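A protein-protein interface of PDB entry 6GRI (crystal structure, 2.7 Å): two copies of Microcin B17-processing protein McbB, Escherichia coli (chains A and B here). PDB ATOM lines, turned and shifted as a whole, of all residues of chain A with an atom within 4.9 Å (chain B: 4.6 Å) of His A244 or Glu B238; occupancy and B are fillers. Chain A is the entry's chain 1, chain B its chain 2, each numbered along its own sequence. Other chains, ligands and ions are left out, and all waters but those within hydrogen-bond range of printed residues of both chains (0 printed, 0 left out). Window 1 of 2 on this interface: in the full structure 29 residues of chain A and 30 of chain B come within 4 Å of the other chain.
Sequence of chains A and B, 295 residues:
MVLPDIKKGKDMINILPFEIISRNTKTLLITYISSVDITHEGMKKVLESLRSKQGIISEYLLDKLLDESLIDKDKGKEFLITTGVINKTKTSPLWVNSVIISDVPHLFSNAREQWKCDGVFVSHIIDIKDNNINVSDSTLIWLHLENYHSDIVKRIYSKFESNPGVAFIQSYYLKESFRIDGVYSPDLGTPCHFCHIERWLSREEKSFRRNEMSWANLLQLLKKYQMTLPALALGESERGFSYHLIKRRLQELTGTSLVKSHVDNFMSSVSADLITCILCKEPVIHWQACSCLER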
ATOM      1  N   ASP A 118      10.106  -8.378   5.359  1.00  0.00           N
ATOM      2  CA  ASP A 118       9.083  -9.404   5.592  1.00  0.00           C
ATOM      3  C   ASP A 118       7.689  -8.954   5.153  1.00  0.00           C
ATOM      4  O   ASP A 118       6.715  -9.697   5.320  1.00  0.00           O
ATOM      5  CB  ASP A 118       9.080  -9.799   7.063  1.00  0.00           C
ATOM      6  CG  ASP A 118      10.388 -10.416   7.486  1.00  0.00           C
ATOM      7  OD1 ASP A 118      10.607 -11.584   7.099  1.00  0.00           O
ATOM      8  OD2 ASP A 118      11.188  -9.731   8.177  1.00  0.00           O
ATOM      9  N   GLY A 240      14.854 -13.222  21.898  1.00  0.00           N
ATOM     10  CA  GLY A 240      15.148 -13.500  20.490  1.00  0.00           C
ATOM     11  C   GLY A 240      14.149 -14.456  19.873  1.00  0.00           C
ATOM     12  O   GLY A 240      13.770 -14.297  18.714  1.00  0.00           O
ATOM     13  N   PHE A 241      13.729 -15.442  20.669  1.00  0.00           N
ATOM     14  CA  PHE A 241      12.657 -16.378  20.308  1.00  0.00           C
ATOM     15  C   PHE A 241      11.345 -15.617  20.151  1.00  0.00           C
ATOM     16  O   PHE A 241      10.675 -15.727  19.125  1.00  0.00           O
ATOM     17  CB  PHE A 241      12.523 -17.448  21.398  1.00  0.00           C
ATOM     18  CG  PHE A 241      11.666 -18.622  21.021  1.00  0.00           C
ATOM     19  CD1 PHE A 241      12.195 -19.678  20.282  1.00  0.00           C
ATOM     20  CD2 PHE A 241      10.350 -18.706  21.450  1.00  0.00           C
ATOM     21  CE1 PHE A 241      11.420 -20.782  19.959  1.00  0.00           C
ATOM     22  CE2 PHE A 241       9.566 -19.807  21.125  1.00  0.00           C
ATOM     23  CZ  PHE A 241      10.098 -20.846  20.378  1.00  0.00           C
ATOM     24  N   SER A 242      11.015 -14.823  21.166  1.00  0.00           N
ATOM     25  CA  SER A 242       9.772 -14.053  21.193  1.00  0.00           C
ATOM     26  C   SER A 242       9.665 -13.037  20.040  1.00  0.00           C
ATOM     27  O   SER A 242       8.612 -12.903  19.403  1.00  0.00           O
ATOM     28  CB  SER A 242       9.630 -13.350  22.553  1.00  0.00           C
ATOM     29  OG  SER A 242       9.750 -14.278  23.633  1.00  0.00           O
ATOM     30  N   TYR A 243      10.768 -12.352  19.762  1.00  0.00           N
ATOM     31  CA  TYR A 243      10.843 -11.387  18.655  1.00  0.00           C
ATOM     32  C   TYR A 243      10.476 -12.041  17.318  1.00  0.00           C
ATOM     33  O   TYR A 243       9.733 -11.462  16.527  1.00  0.00           O
ATOM     34  CB  TYR A 243      12.256 -10.795  18.603  1.00  0.00           C
ATOM     35  CG  TYR A 243      12.498  -9.585  17.706  1.00  0.00           C
ATOM     36  CD1 TYR A 243      11.927  -8.341  17.986  1.00  0.00           C
ATOM     37  CD2 TYR A 243      13.380  -9.670  16.626  1.00  0.00           C
ATOM     38  CE1 TYR A 243      12.200  -7.238  17.189  1.00  0.00           C
ATOM     39  CE2 TYR A 243      13.652  -8.580  15.823  1.00  0.00           C
ATOM     40  CZ  TYR A 243      13.065  -7.366  16.099  1.00  0.00           C
ATOM     41  OH  TYR A 243      13.372  -6.297  15.280  1.00  0.00           O
ATOM     42  N   HIS A 244      10.979 -13.255  17.089  1.00  0.00           N
ATOM     43  CA  HIS A 244      10.736 -13.964  15.840  1.00  0.00           C
ATOM     44  C   HIS A 244       9.287 -14.425  15.706  1.00  0.00           C
ATOM     45  O   HIS A 244       8.698 -14.313  14.623  1.00  0.00           O
ATOM     46  CB  HIS A 244      11.694 -15.158  15.707  1.00  0.00           C
ATOM     47  CG  HIS A 244      11.561 -15.893  14.407  1.00  0.00           C
ATOM     48  ND1 HIS A 244      11.720 -15.276  13.185  1.00  0.00           N
ATOM     49  CD2 HIS A 244      11.237 -17.181  14.140  1.00  0.00           C
ATOM     50  CE1 HIS A 244      11.508 -16.155  12.221  1.00  0.00           C
ATOM     51  NE2 HIS A 244      11.223 -17.322  12.774  1.00  0.00           N
ATOM     52  N   LEU A 245       8.715 -14.949  16.796  1.00  0.00           N
ATOM     53  CA  LEU A 245       7.299 -15.346  16.805  1.00  0.00           C
ATOM     54  C   LEU A 245       6.365 -14.159  16.570  1.00  0.00           C
ATOM     55  O   LEU A 245       5.381 -14.288  15.825  1.00  0.00           O
ATOM     56  CB  LEU A 245       6.914 -16.037  18.112  1.00  0.00           C
ATOM     57  CG  LEU A 245       7.556 -17.381  18.474  1.00  0.00           C
ATOM     58  CD1 LEU A 245       6.745 -18.042  19.576  1.00  0.00           C
ATOM     59  CD2 LEU A 245       7.669 -18.319  17.285  1.00  0.00           C
ATOM     60  N   ILE A 246       6.681 -13.017  17.191  1.00  0.00           N
ATOM     61  CA  ILE A 246       5.913 -11.789  16.988  1.00  0.00           C
ATOM     62  C   ILE A 246       5.953 -11.394  15.514  1.00  0.00           C
ATOM     63  O   ILE A 246       4.927 -11.055  14.934  1.00  0.00           O
ATOM     64  CB  ILE A 246       6.439 -10.611  17.849  1.00  0.00           C
ATOM     65  CG1 ILE A 246       6.230 -10.877  19.346  1.00  0.00           C
ATOM     66  CG2 ILE A 246       5.759  -9.288  17.474  1.00  0.00           C
ATOM     67  CD1 ILE A 246       7.206 -10.130  20.230  1.00  0.00           C
ATOM     68  N   LYS A 247       7.133 -11.428  14.911  1.00  0.00           N
ATOM     69  CA  LYS A 247       7.272 -11.034  13.513  1.00  0.00           C
ATOM     70  C   LYS A 247       6.437 -11.933  12.619  1.00  0.00           C
ATOM     71  O   LYS A 247       5.677 -11.451  11.767  1.00  0.00           O
ATOM     72  CB  LYS A 247       8.727 -11.110  13.074  1.00  0.00           C
ATOM     73  CG  LYS A 247       8.975 -10.580  11.676  1.00  0.00           C
ATOM     74  CD  LYS A 247      10.385 -10.881  11.231  1.00  0.00           C
ATOM     75  CE  LYS A 247      10.476 -12.249  10.584  1.00  0.00           C
ATOM     76  NZ  LYS A 247      11.828 -12.468  10.013  1.00  0.00           N
ATOM     77  N   ARG A 248       6.584 -13.242  12.817  1.00  0.00           N
ATOM     78  CA  ARG A 248       5.902 -14.218  11.968  1.00  0.00           C
ATOM     79  C   ARG A 248       4.406 -14.143  12.111  1.00  0.00           C
ATOM     80  O   ARG A 248       3.690 -14.310  11.128  1.00  0.00           O
ATOM     81  CB  ARG A 248       6.382 -15.634  12.251  1.00  0.00           C
ATOM     82  CG  ARG A 248       7.804 -15.917  11.800  1.00  0.00           C
ATOM     83  CD  ARG A 248       7.983 -15.623  10.324  1.00  0.00           C
ATOM     84  NE  ARG A 248       9.157 -16.259   9.758  1.00  0.00           N
ATOM     85  CZ  ARG A 248       9.764 -15.877   8.635  1.00  0.00           C
ATOM     86  NH1 ARG A 248       9.333 -14.834   7.928  1.00  0.00           N
ATOM     87  NH2 ARG A 248      10.833 -16.544   8.218  1.00  0.00           N
ATOM     88  N   ALA B 233      18.231 -15.356   3.351  1.00  0.00           N
ATOM     89  CA  ALA B 233      17.857 -14.044   3.877  1.00  0.00           C
ATOM     90  C   ALA B 233      17.560 -14.041   5.375  1.00  0.00           C
ATOM     91  O   ALA B 233      16.506 -13.573   5.801  1.00  0.00           O
ATOM     92  CB  ALA B 233      16.684 -13.479   3.086  1.00  0.00           C
ATOM     93  N   LEU B 234      18.510 -14.548   6.162  1.00  0.00           N
ATOM     94  CA  LEU B 234      18.410 -14.522   7.620  1.00  0.00           C
ATOM     95  C   LEU B 234      18.522 -13.115   8.145  1.00  0.00           C
ATOM     96  O   LEU B 234      19.476 -12.420   7.835  1.00  0.00           O
ATOM     97  CB  LEU B 234      19.522 -15.334   8.276  1.00  0.00           C
ATOM     98  CG  LEU B 234      19.527 -16.826   8.002  1.00  0.00           C
ATOM     99  CD1 LEU B 234      20.567 -17.480   8.894  1.00  0.00           C
ATOM    100  CD2 LEU B 234      18.151 -17.449   8.201  1.00  0.00           C
ATOM    101  N   GLY B 235      17.543 -12.712   8.943  1.00  0.00           N
ATOM    102  CA  GLY B 235      17.590 -11.445   9.658  1.00  0.00           C
ATOM    103  C   GLY B 235      17.891 -11.703  11.116  1.00  0.00           C
ATOM    104  O   GLY B 235      18.222 -12.832  11.501  1.00  0.00           O
ATOM    105  N   GLU B 236      17.769 -10.648  11.921  1.00  0.00           N
ATOM    106  CA  GLU B 236      18.049 -10.707  13.358  1.00  0.00           C
ATOM    107  C   GLU B 236      17.144 -11.710  14.042  1.00  0.00           C
ATOM    108  O   GLU B 236      17.624 -12.545  14.810  1.00  0.00           O
ATOM    109  CB  GLU B 236      17.857  -9.331  14.006  1.00  0.00           C
ATOM    110  CG  GLU B 236      18.369  -9.226  15.439  1.00  0.00           C
ATOM    111  CD  GLU B 236      18.322  -7.803  15.972  1.00  0.00           C
ATOM    112  OE1 GLU B 236      17.321  -7.101  15.703  1.00  0.00           O
ATOM    113  OE2 GLU B 236      19.287  -7.388  16.657  1.00  0.00           O
ATOM    114  N   SER B 237      15.844 -11.623  13.737  1.00  0.00           N
ATOM    115  CA  SER B 237      14.824 -12.470  14.364  1.00  0.00           C
ATOM    116  C   SER B 237      15.049 -13.961  14.096  1.00  0.00           C
ATOM    117  O   SER B 237      14.869 -14.777  15.005  1.00  0.00           O
ATOM    118  CB  SER B 237      13.402 -12.043  13.955  1.00  0.00           C
ATOM    119  OG  SER B 237      13.007 -12.553  12.693  1.00  0.00           O
ATOM    120  N   GLU B 238      15.460 -14.311  12.872  1.00  0.00           N
ATOM    121  CA  GLU B 238      15.790 -15.706  12.545  1.00  0.00           C
ATOM    122  C   GLU B 238      16.998 -16.170  13.338  1.00  0.00           C
ATOM    123  O   GLU B 238      17.003 -17.282  13.850  1.00  0.00           O
ATOM    124  CB  GLU B 238      16.065 -15.905  11.059  1.00  0.00           C
ATOM    125  CG  GLU B 238      14.824 -16.026  10.184  1.00  0.00           C
ATOM    126  CD  GLU B 238      14.186 -14.697   9.825  1.00  0.00           C
ATOM    127  OE1 GLU B 238      14.847 -13.636   9.928  1.00  0.00           O
ATOM    128  OE2 GLU B 238      13.002 -14.716   9.415  1.00  0.00           O
ATOM    129  N   ARG B 239      18.015 -15.313  13.433  1.00  0.00           N
ATOM    130  CA  ARG B 239      19.199 -15.601  14.250  1.00  0.00           C
ATOM    131  C   ARG B 239      18.877 -15.741  15.733  1.00  0.00           C
ATOM    132  O   ARG B 239      19.477 -16.575  16.423  1.00  0.00           O
ATOM    133  CB  ARG B 239      20.275 -14.535  14.058  1.00  0.00           C
ATOM    134  CG  ARG B 239      20.983 -14.632  12.722  1.00  0.00           C
ATOM    135  CD  ARG B 239      22.198 -13.724  12.659  1.00  0.00           C
ATOM    136  NE  ARG B 239      22.741 -13.678  11.303  1.00  0.00           N
ATOM    137  CZ  ARG B 239      22.200 -13.022  10.272  1.00  0.00           C
ATOM    138  NH1 ARG B 239      21.075 -12.323  10.411  1.00  0.00           N
ATOM    139  NH2 ARG B 239      22.793 -13.063   9.079  1.00  0.00           N
ATOM    140  N   GLY B 240      17.936 -14.924  16.215  1.00  0.00           N
ATOM    141  CA  GLY B 240      17.432 -15.027  17.588  1.00  0.00           C
ATOM    142  C   GLY B 240      16.717 -16.339  17.851  1.00  0.00           C
ATOM    143  O   GLY B 240      16.945 -16.980  18.876  1.00  0.00           O
ATOM    144  N   PHE B 241      15.848 -16.725  16.919  1.00  0.00           N
ATOM    145  CA  PHE B 241      15.161 -18.020  16.954  1.00  0.00           C
ATOM    146  C   PHE B 241      16.178 -19.152  16.975  1.00  0.00           C
ATOM    147  O   PHE B 241      16.039 -20.088  17.754  1.00  0.00           O
ATOM    148  CB  PHE B 241      14.244 -18.152  15.735  1.00  0.00           C
ATOM    149  CG  PHE B 241      13.376 -19.384  15.728  1.00  0.00           C
ATOM    150  CD1 PHE B 241      12.333 -19.528  16.631  1.00  0.00           C
ATOM    151  CD2 PHE B 241      13.560 -20.371  14.775  1.00  0.00           C
ATOM    152  CE1 PHE B 241      11.515 -20.652  16.593  1.00  0.00           C
ATOM    153  CE2 PHE B 241      12.750 -21.491  14.737  1.00  0.00           C
ATOM    154  CZ  PHE B 241      11.729 -21.635  15.647  1.00  0.00           C
ATOM    155  N   SER B 242      17.210 -19.046  16.137  1.00  0.00           N
ATOM    156  CA  SER B 242      18.298 -20.039  16.103  1.00  0.00           C
ATOM    157  C   SER B 242      19.128 -20.037  17.396  1.00  0.00           C
ATOM    158  O   SER B 242      19.427 -21.097  17.941  1.00  0.00           O
ATOM    159  CB  SER B 242      19.205 -19.818  14.881  1.00  0.00           C
ATOM    160  OG  SER B 242      18.538 -20.149  13.667  1.00  0.00           O
ATOM    161  N   LEU B 274      11.559 -22.102   9.754  1.00  0.00           N
ATOM    162  CA  LEU B 274      11.715 -20.705  10.148  1.00  0.00           C
ATOM    163  C   LEU B 274      10.516 -19.822   9.826  1.00  0.00           C
ATOM    164  O   LEU B 274      10.389 -18.729  10.388  1.00  0.00           O
ATOM    165  CB  LEU B 274      12.951 -20.108   9.486  1.00  0.00           C
ATOM    166  CG  LEU B 274      14.280 -20.750   9.847  1.00  0.00           C
ATOM    167  CD1 LEU B 274      15.397 -19.947   9.196  1.00  0.00           C
ATOM    168  CD2 LEU B 274      14.488 -20.824  11.357  1.00  0.00           C
ATOM    169  N   CYS B 277       7.731 -21.609  12.463  1.00  0.00           N
ATOM    170  CA  CYS B 277       8.314 -21.790  13.792  1.00  0.00           C
ATOM    171  C   CYS B 277       7.969 -23.138  14.423  1.00  0.00           C
ATOM    172  O   CYS B 277       7.980 -23.277  15.643  1.00  0.00           O
ATOM    173  CB  CYS B 277       7.933 -20.634  14.725  1.00  0.00           C
ATOM    174  SG  CYS B 277       8.258 -19.012  14.013  1.00  0.00           S
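The side-chain hydroxyl (OG) of Ser B237 is in hydrogen-bond range of a ring nitrogen (ND1) of His A244. The side-chain amino group (NZ) of Lys A247 lies within salt-bridge range of the side-chain carboxylate (OE2) of Glu B238 (2.6 Å). The guanidinium group (NE) of Arg A248 sits at hydrogen-bond distance from the backbone carbonyl oxygen (O) of Leu B274. A ring nitrogen (NE2) of His A244 lies close to the side-chain sulfur (SG) of Cys B277 (3.6 Å). A ring nitrogen (NE2) of His A244 sits at hydrogen-bond distance from the backbone carbonyl oxygen (O) of Leu B274 (2.9 Å). The guanidinium group (NH2) of Arg A248 is in salt-bridge range of the side-chain carboxylate (OE2) of Glu B238 (3.1 Å). The side-chain amino group (NZ) of Lys A247 sits at hydrogen-bond distance from the side-chain hydroxyl (OG) of Ser B237 (2.9 Å).
Gly B240 touches its own counterpart, Gly A240. Gly A240 touches Phe B241, and with the chains exchanged Phe A241 touches Gly B240. Phe A241 touches its own counterpart, Phe B241. Of the 18 pairs that touch across the chains among the printed residues, 4 have their exchanged pair printed and touching as well.
Printed residues of chain A that touch a printed residue of chain B: Gly A240, Phe A241, Tyr A243, His A244, Leu A245, Lys A247 and Arg A248. Of the 12 printed residues of chain B, 7 touch a printed residue of chain A. Hydrophobic or aromatic side chains of chain B within 4 Å of the printed part of chain A: Phe B241. Among the printed residues, Asp or Glu carboxylates within 4 Å of a Lys or Arg side-chain nitrogen of the other chain: Lys A247 with Glu B238 (2.6 Å) and Arg A248 with Glu B238 (3.1 Å).
Printed residues of chain B within 4 Å of Gly A240: Ser B237 (3.9 Å), Gly B240 (3.7 Å) and Phe B241 (3.7 Å). Of the printed residues of chain B, Phe A241 touches Gly B240 and Phe B241. Of the printed residues of chain B, His A244 touches Ser B237 (3.1 Å), Glu B238 (3.5 Å), Phe B241 (3.5 Å), Leu B274 (2.9 Å) and Cys B277 (3.5 Å). Of the printed residues of chain B, Leu A245 touches Cys B277 (3.4 Å). Glu B238 touches just these residues of chain A: His A244, Lys A247 and Arg A248. Of the printed residues of chain A, Gly B240 touches Gly A240 and Phe A241. The nearest printed residue of chain B that does not touch His A244 is Gly B240 (5.6 Å). The nearest residue of chain A that does not touch Glu B238 is Asp A118 (4.6 Å).
OD1 of Asp A118 is in salt-bridge range of NZ of Lys A247, at 3.3 Å. The side-chain carboxylate (OE1) of Glu B238 sits at hydrogen-bond distance from the backbone NH (N) of Gly B235 (3.0 Å). The side-chain hydroxyl (OG) of Ser B237 is in hydrogen-bond range of the side-chain carboxylate (OE1) of Glu B238 (3.5 Å). The backbone carbonyl oxygen of Glu B238 sits at hydrogen-bond distance from the side-chain hydroxyl of Ser B242, 3.3 Å away. NH1 of Arg A248 lies within salt-bridge range of OD1 of Asp A118, 3.6 Å away.
Among the printed residues, merely in contact across the chains: Phe A241 with Phe B241 (3.4 Å), Leu A245 with Cys B277 (3.4 Å), His A244 with Phe B241 (3.5 Å), His A244 with Glu B238 (3.5 Å), Tyr A243 with Ser B237 (3.6 Å), Gly A240 with Phe B241 (3.7 Å), Gly A240 with Gly B240 (3.7 Å), Arg A248 with Cys B277 (3.8 Å), Gly A240 with Ser B237 (3.9 Å), Tyr A243 with Glu B236 (3.96 Å) and Phe A241 with Gly B240 (3.99 Å).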
